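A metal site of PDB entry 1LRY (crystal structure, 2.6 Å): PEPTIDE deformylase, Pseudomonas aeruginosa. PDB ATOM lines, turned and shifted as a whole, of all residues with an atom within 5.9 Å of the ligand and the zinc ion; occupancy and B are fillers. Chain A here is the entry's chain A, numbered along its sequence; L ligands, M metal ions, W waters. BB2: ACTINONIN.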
ATOM      1  N   PRO A  42       0.243  10.422  14.784  1.00  0.00           N
ATOM      2  CA  PRO A  42       0.566  11.606  13.989  1.00  0.00           C
ATOM      3  C   PRO A  42       0.938  12.812  14.853  1.00  0.00           C
ATOM      4  O   PRO A  42       0.410  13.000  15.950  1.00  0.00           O
ATOM      5  CB  PRO A  42      -0.751  11.867  13.266  1.00  0.00           C
ATOM      6  CG  PRO A  42      -1.742  11.616  14.349  1.00  0.00           C
ATOM      7  CD  PRO A  42      -1.213  10.365  15.056  1.00  0.00           C
ATOM      8  N   GLY A  43       1.854  13.631  14.326  1.00  0.00           N
ATOM      9  CA  GLY A  43       2.285  14.826  15.014  1.00  0.00           C
ATOM     10  C   GLY A  43       2.448  15.945  14.001  1.00  0.00           C
ATOM     11  O   GLY A  43       2.462  15.680  12.786  1.00  0.00           O
ATOM     12  N   ILE A  44       2.536  17.189  14.476  1.00  0.00           N
ATOM     13  CA  ILE A  44       2.725  18.338  13.577  1.00  0.00           C
ATOM     14  C   ILE A  44       4.182  18.792  13.526  1.00  0.00           C
ATOM     15  O   ILE A  44       4.488  19.831  12.946  1.00  0.00           O
ATOM     16  CB  ILE A  44       1.801  19.536  13.933  1.00  0.00           C
ATOM     17  CG1 ILE A  44       2.269  20.203  15.228  1.00  0.00           C
ATOM     18  CG2 ILE A  44       0.361  19.058  14.059  1.00  0.00           C
ATOM     19  CD1 ILE A  44       1.397  21.356  15.682  1.00  0.00           C
ATOM     20  N   GLY A  45       5.065  17.995  14.113  1.00  0.00           N
ATOM     21  CA  GLY A  45       6.495  18.301  14.149  1.00  0.00           C
ATOM     22  C   GLY A  45       7.307  17.167  14.738  1.00  0.00           C
ATOM     23  O   GLY A  45       6.757  16.304  15.413  1.00  0.00           O
ATOM     24  N   LEU A  46       8.616  17.171  14.504  1.00  0.00           N
ATOM     25  CA  LEU A  46       9.521  16.125  14.992  1.00  0.00           C
ATOM     26  C   LEU A  46      10.988  16.523  14.829  1.00  0.00           C
ATOM     27  O   LEU A  46      11.399  16.952  13.754  1.00  0.00           O
ATOM     28  CB  LEU A  46       9.280  14.805  14.232  1.00  0.00           C
ATOM     29  CG  LEU A  46       9.959  13.507  14.679  1.00  0.00           C
ATOM     30  CD1 LEU A  46       9.133  12.812  15.748  1.00  0.00           C
ATOM     31  CD2 LEU A  46      10.114  12.563  13.501  1.00  0.00           C
ATOM     32  N   ALA A  47      11.768  16.360  15.891  1.00  0.00           N
ATOM     33  CA  ALA A  47      13.198  16.667  15.862  1.00  0.00           C
ATOM     34  C   ALA A  47      13.961  15.343  15.895  1.00  0.00           C
ATOM     35  O   ALA A  47      13.502  14.363  16.492  1.00  0.00           O
ATOM     36  CB  ALA A  47      13.582  17.515  17.029  1.00  0.00           C
ATOM     37  N   GLN A  50      14.240  12.776  18.981  1.00  0.00           N
ATOM     38  CA  GLN A  50      13.121  11.915  19.336  1.00  0.00           C
ATOM     39  C   GLN A  50      13.224  10.522  18.749  1.00  0.00           C
ATOM     40  O   GLN A  50      12.577   9.597  19.256  1.00  0.00           O
ATOM     41  CB  GLN A  50      11.795  12.527  18.881  1.00  0.00           C
ATOM     42  CG  GLN A  50      11.411  13.863  19.506  1.00  0.00           C
ATOM     43  CD  GLN A  50       9.963  14.262  19.214  1.00  0.00           C
ATOM     44  OE1 GLN A  50       9.673  14.954  18.234  1.00  0.00           O
ATOM     45  NE2 GLN A  50       9.053  13.833  20.082  1.00  0.00           N
ATOM     46  N   TYR A  87      -0.124  27.572  26.130  1.00  0.00           N
ATOM     47  CA  TYR A  87      -0.631  26.600  25.171  1.00  0.00           C
ATOM     48  C   TYR A  87      -0.525  25.171  25.703  1.00  0.00           C
ATOM     49  O   TYR A  87       0.521  24.765  26.181  1.00  0.00           O
ATOM     50  CB  TYR A  87       0.135  26.708  23.847  1.00  0.00           C
ATOM     51  CG  TYR A  87      -0.544  26.040  22.682  1.00  0.00           C
ATOM     52  CD1 TYR A  87      -1.366  26.764  21.823  1.00  0.00           C
ATOM     53  CD2 TYR A  87      -0.393  24.668  22.446  1.00  0.00           C
ATOM     54  CE1 TYR A  87      -2.019  26.143  20.759  1.00  0.00           C
ATOM     55  CE2 TYR A  87      -1.048  24.037  21.384  1.00  0.00           C
ATOM     56  CZ  TYR A  87      -1.855  24.786  20.547  1.00  0.00           C
ATOM     57  OH  TYR A  87      -2.513  24.169  19.495  1.00  0.00           O
ATOM     58  N   GLN A  88      -1.613  24.419  25.591  1.00  0.00           N
ATOM     59  CA  GLN A  88      -1.645  23.042  26.058  1.00  0.00           C
ATOM     60  C   GLN A  88      -0.957  22.144  25.050  1.00  0.00           C
ATOM     61  O   GLN A  88      -1.564  21.702  24.082  1.00  0.00           O
ATOM     62  CB  GLN A  88      -3.088  22.593  26.278  1.00  0.00           C
ATOM     63  CG  GLN A  88      -3.225  21.282  26.992  1.00  0.00           C
ATOM     64  CD  GLN A  88      -4.681  20.907  27.201  1.00  0.00           C
ATOM     65  OE1 GLN A  88      -5.389  20.587  26.248  1.00  0.00           O
ATOM     66  NE2 GLN A  88      -5.134  20.965  28.450  1.00  0.00           N
ATOM     67  N   GLU A  89       0.330  21.897  25.275  1.00  0.00           N
ATOM     68  CA  GLU A  89       1.157  21.085  24.401  1.00  0.00           C
ATOM     69  C   GLU A  89       1.255  19.622  24.779  1.00  0.00           C
ATOM     70  O   GLU A  89       1.311  19.273  25.954  1.00  0.00           O
ATOM     71  CB  GLU A  89       2.587  21.638  24.373  1.00  0.00           C
ATOM     72  CG  GLU A  89       2.705  23.126  24.090  1.00  0.00           C
ATOM     73  CD  GLU A  89       4.135  23.636  24.203  1.00  0.00           C
ATOM     74  OE1 GLU A  89       5.086  22.832  24.114  1.00  0.00           O
ATOM     75  OE2 GLU A  89       4.302  24.858  24.377  1.00  0.00           O
ATOM     76  N   GLY A  90       1.351  18.780  23.756  1.00  0.00           N
ATOM     77  CA  GLY A  90       1.501  17.351  23.929  1.00  0.00           C
ATOM     78  C   GLY A  90       2.792  17.001  23.218  1.00  0.00           C
ATOM     79  O   GLY A  90       3.359  17.842  22.519  1.00  0.00           O
ATOM     80  N   CYS A  91       3.262  15.759  23.352  1.00  0.00           N
ATOM     81  CA  CYS A  91       4.505  15.364  22.704  1.00  0.00           C
ATOM     82  C   CYS A  91       4.473  13.895  22.408  1.00  0.00           C
ATOM     83  O   CYS A  91       3.936  13.103  23.183  1.00  0.00           O
ATOM     84  CB  CYS A  91       5.697  15.697  23.612  1.00  0.00           C
ATOM     85  SG  CYS A  91       7.334  15.178  23.007  1.00  0.00           S
ATOM     86  N   LEU A  92       5.052  13.516  21.277  1.00  0.00           N
ATOM     87  CA  LEU A  92       5.095  12.125  20.868  1.00  0.00           C
ATOM     88  C   LEU A  92       6.040  11.325  21.771  1.00  0.00           C
ATOM     89  O   LEU A  92       6.012  10.098  21.785  1.00  0.00           O
ATOM     90  CB  LEU A  92       5.537  11.991  19.398  1.00  0.00           C
ATOM     91  CG  LEU A  92       4.700  12.694  18.318  1.00  0.00           C
ATOM     92  CD1 LEU A  92       5.245  12.356  16.949  1.00  0.00           C
ATOM     93  CD2 LEU A  92       3.231  12.305  18.437  1.00  0.00           C
ATOM     94  N   SER A  93       6.869  12.038  22.524  1.00  0.00           N
ATOM     95  CA  SER A  93       7.802  11.378  23.423  1.00  0.00           C
ATOM     96  C   SER A  93       7.272  11.371  24.861  1.00  0.00           C
ATOM     97  O   SER A  93       7.840  10.728  25.739  1.00  0.00           O
ATOM     98  CB  SER A  93       9.171  12.028  23.321  1.00  0.00           C
ATOM     99  OG  SER A  93       9.652  11.922  21.972  1.00  0.00           O
ATOM    100  N   TYR A  98      -0.731  16.155  28.384  1.00  0.00           N
ATOM    101  CA  TYR A  98      -0.781  17.478  27.753  1.00  0.00           C
ATOM    102  C   TYR A  98      -0.856  18.544  28.828  1.00  0.00           C
ATOM    103  O   TYR A  98      -1.844  18.644  29.559  1.00  0.00           O
ATOM    104  CB  TYR A  98      -1.999  17.589  26.847  1.00  0.00           C
ATOM    105  CG  TYR A  98      -2.191  16.365  25.980  1.00  0.00           C
ATOM    106  CD1 TYR A  98      -3.030  15.330  26.379  1.00  0.00           C
ATOM    107  CD2 TYR A  98      -1.480  16.226  24.787  1.00  0.00           C
ATOM    108  CE1 TYR A  98      -3.163  14.179  25.616  1.00  0.00           C
ATOM    109  CE2 TYR A  98      -1.603  15.081  24.018  1.00  0.00           C
ATOM    110  CZ  TYR A  98      -2.444  14.054  24.438  1.00  0.00           C
ATOM    111  OH  TYR A  98      -2.565  12.901  23.681  1.00  0.00           O
ATOM    112  N   LEU A 126       0.994  28.983  16.048  1.00  0.00           N
ATOM    113  CA  LEU A 126       1.470  27.612  16.220  1.00  0.00           C
ATOM    114  C   LEU A 126       2.932  27.348  15.839  1.00  0.00           C
ATOM    115  O   LEU A 126       3.595  26.536  16.473  1.00  0.00           O
ATOM    116  CB  LEU A 126       0.527  26.669  15.475  1.00  0.00           C
ATOM    117  CG  LEU A 126       0.489  25.177  15.836  1.00  0.00           C
ATOM    118  CD1 LEU A 126       0.407  24.979  17.343  1.00  0.00           C
ATOM    119  CD2 LEU A 126      -0.710  24.550  15.148  1.00  0.00           C
ATOM    120  N   VAL A 129       5.400  28.410  18.746  1.00  0.00           N
ATOM    121  CA  VAL A 129       5.346  27.395  19.792  1.00  0.00           C
ATOM    122  C   VAL A 129       6.056  26.114  19.365  1.00  0.00           C
ATOM    123  O   VAL A 129       6.923  25.591  20.074  1.00  0.00           O
ATOM    124  CB  VAL A 129       3.880  27.044  20.143  1.00  0.00           C
ATOM    125  CG1 VAL A 129       3.828  26.142  21.351  1.00  0.00           C
ATOM    126  CG2 VAL A 129       3.093  28.316  20.416  1.00  0.00           C
ATOM    127  N   CYS A 130       5.738  25.657  18.162  1.00  0.00           N
ATOM    128  CA  CYS A 130       6.328  24.438  17.649  1.00  0.00           C
ATOM    129  C   CYS A 130       7.835  24.457  17.496  1.00  0.00           C
ATOM    130  O   CYS A 130       8.497  23.517  17.950  1.00  0.00           O
ATOM    131  CB  CYS A 130       5.672  24.032  16.341  1.00  0.00           C
ATOM    132  SG  CYS A 130       6.103  22.369  15.834  1.00  0.00           S
ATOM    133  N   HIS A 133       9.250  24.222  20.804  1.00  0.00           N
ATOM    134  CA  HIS A 133       9.075  22.883  21.365  1.00  0.00           C
ATOM    135  C   HIS A 133      10.066  21.900  20.747  1.00  0.00           C
ATOM    136  O   HIS A 133      10.470  20.946  21.396  1.00  0.00           O
ATOM    137  CB  HIS A 133       7.628  22.440  21.144  1.00  0.00           C
ATOM    138  CG  HIS A 133       7.344  21.032  21.576  1.00  0.00           C
ATOM    139  ND1 HIS A 133       6.672  20.727  22.740  1.00  0.00           N
ATOM    140  CD2 HIS A 133       7.567  19.840  20.964  1.00  0.00           C
ATOM    141  CE1 HIS A 133       6.486  19.424  22.813  1.00  0.00           C
ATOM    142  NE2 HIS A 133       7.028  18.859  21.747  1.00  0.00           N
ATOM    143  N   GLU A 134      10.486  22.174  19.516  1.00  0.00           N
ATOM    144  CA  GLU A 134      11.426  21.327  18.780  1.00  0.00           C
ATOM    145  C   GLU A 134      12.882  21.636  19.059  1.00  0.00           C
ATOM    146  O   GLU A 134      13.739  20.752  18.992  1.00  0.00           O
ATOM    147  CB  GLU A 134      11.189  21.437  17.256  1.00  0.00           C
ATOM    148  CG  GLU A 134       9.798  21.031  16.774  1.00  0.00           C
ATOM    149  CD  GLU A 134       9.415  19.616  17.149  1.00  0.00           C
ATOM    150  OE1 GLU A 134      10.306  18.741  17.242  1.00  0.00           O
ATOM    151  OE2 GLU A 134       8.211  19.363  17.340  1.00  0.00           O
ATOM    152  N   HIS A 137      14.002  19.876  22.124  1.00  0.00           N
ATOM    153  CA  HIS A 137      14.386  18.493  21.873  1.00  0.00           C
ATOM    154  C   HIS A 137      15.874  18.348  21.555  1.00  0.00           C
ATOM    155  O   HIS A 137      16.517  17.381  21.978  1.00  0.00           O
ATOM    156  CB  HIS A 137      13.570  17.909  20.713  1.00  0.00           C
ATOM    157  CG  HIS A 137      12.223  17.406  21.103  1.00  0.00           C
ATOM    158  ND1 HIS A 137      12.049  16.388  22.022  1.00  0.00           N
ATOM    159  CD2 HIS A 137      10.981  17.819  20.757  1.00  0.00           C
ATOM    160  CE1 HIS A 137      10.762  16.201  22.232  1.00  0.00           C
ATOM    161  NE2 HIS A 137      10.085  17.056  21.484  1.00  0.00           N
HETATM  162  C5  BB2 L   1       5.017  16.607  18.297  1.00  0.00           C
HETATM  163  C3  BB2 L   1       6.333  16.475  19.058  1.00  0.00           C
HETATM  164  O4  BB2 L   1       6.421  15.642  19.996  1.00  0.00           O
HETATM  165  N1  BB2 L   1       7.337  17.238  18.618  1.00  0.00           N
HETATM  166  O2  BB2 L   1       8.614  17.274  19.171  1.00  0.00           O
HETATM  167  C6  BB2 L   1       4.194  17.746  18.878  1.00  0.00           C
HETATM  168  C12 BB2 L   1       2.716  17.490  18.586  1.00  0.00           C
HETATM  169  O13 BB2 L   1       2.346  17.165  17.464  1.00  0.00           O
HETATM  170  C7  BB2 L   1       4.598  19.080  18.249  1.00  0.00           C
HETATM  171  C8  BB2 L   1       4.741  20.241  19.226  1.00  0.00           C
HETATM  172  C9  BB2 L   1       3.480  20.459  20.052  1.00  0.00           C
HETATM  173  C10 BB2 L   1       3.031  21.909  19.985  1.00  0.00           C
HETATM  174  C11 BB2 L   1       4.186  22.838  20.163  1.00  0.00           C
HETATM  175  N14 BB2 L   1       1.887  17.637  19.616  1.00  0.00           N
HETATM  176  C15 BB2 L   1       0.449  17.458  19.500  1.00  0.00           C
HETATM  177  C16 BB2 L   1      -0.036  16.181  20.260  1.00  0.00           C
HETATM  178  C18 BB2 L   1       0.758  14.965  19.829  1.00  0.00           C
HETATM  179  C17 BB2 L   1      -1.499  15.949  19.990  1.00  0.00           C
HETATM  180  C19 BB2 L   1      -0.155  18.698  20.147  1.00  0.00           C
HETATM  181  O20 BB2 L   1       0.208  19.036  21.269  1.00  0.00           O
HETATM  182  N21 BB2 L   1      -1.043  19.414  19.426  1.00  0.00           N
HETATM  183  C22 BB2 L   1      -1.695  20.629  19.922  1.00  0.00           C
HETATM  184  C23 BB2 L   1      -1.366  19.211  18.005  1.00  0.00           C
HETATM  185  C24 BB2 L   1      -1.631  20.619  17.542  1.00  0.00           C
HETATM  186  C25 BB2 L   1      -2.431  21.156  18.685  1.00  0.00           C
HETATM  187  C26 BB2 L   1      -2.628  20.116  21.027  1.00  0.00           C
HETATM  188  O27 BB2 L   1      -3.578  21.104  21.374  1.00  0.00           O
HETATM  189 ZN    ZN M   1       7.838  16.820  21.180  1.00  0.00          ZN
HETATM  190  O   HOH W   1      -5.584  23.037  21.006  1.00  0.00           O
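A ring nitrogen (ND1) of His 133 sits at hydrogen-bond distance from the side-chain carboxylate (OE1) of Glu 89. NE2 of Gln 50 lies close to SG of Cys 91 (3.6 Å). SG of Cys 91 sits close to N of Ser 93 (3.2 Å). The backbone NH of Ala 47 sits at hydrogen-bond distance from the side-chain carboxylate of Glu 134. OG of Ser 93 sits at hydrogen-bond distance from NE2 of Gln 50 (2.8 Å). N of Ala 47 sits at hydrogen-bond distance from OE1 of Gln 50 (3.4 Å).
Residues that only touch the ligand: Gly 43 (3.4 Å), Tyr 87 (3.1 Å), Glu 89 (3.7 Å), Val 129 (3.5 Å) and Cys 130 (3.7 Å). Along chain A the residues within 4 Å of the ligand span positions 43 to 137.
The zinc ion is bound by O4 of the ligand (2.2 Å), O2 of the ligand (2.2 Å), NE2 of His 133 (2.3 Å), NE2 of His 137 (2.3 Å) and SG of Cys 91 (2.5 Å). The zinc ion has five donor atoms within binding distance.
A nitrogen (N1) of the ligand lies within hydrogen-bond range of the side-chain carboxylate (OE2) of Glu 134 (2.6 Å). OE1 of Gln 50 is in hydrogen-bond range of N1 of the ligand (3.3 Å). The backbone NH (N) of Gly 90 lies within hydrogen-bond range of an oxygen (O20) of the ligand (2.7 Å). The backbone carbonyl oxygen (O) of Gly 90 lies within hydrogen-bond range of a nitrogen (N14) of the ligand (3.3 Å). The backbone NH of Leu 92 lies close to an oxygen (O4) of the ligand (2.8 Å). An oxygen (O13) of the ligand lies within hydrogen-bond range of the backbone NH of Ile 44 (3.0 Å). N1 of the ligand lies close to O of Gly 45 (3.4 Å). O of Gln 88 lies within hydrogen-bond range of O27 of the ligand (3.4 Å).
Residues that only touch the zinc ion: Gln 50 (3.4 Å). The nearest printed residue that does not touch the zinc ion is Leu 92 (4.3 Å).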
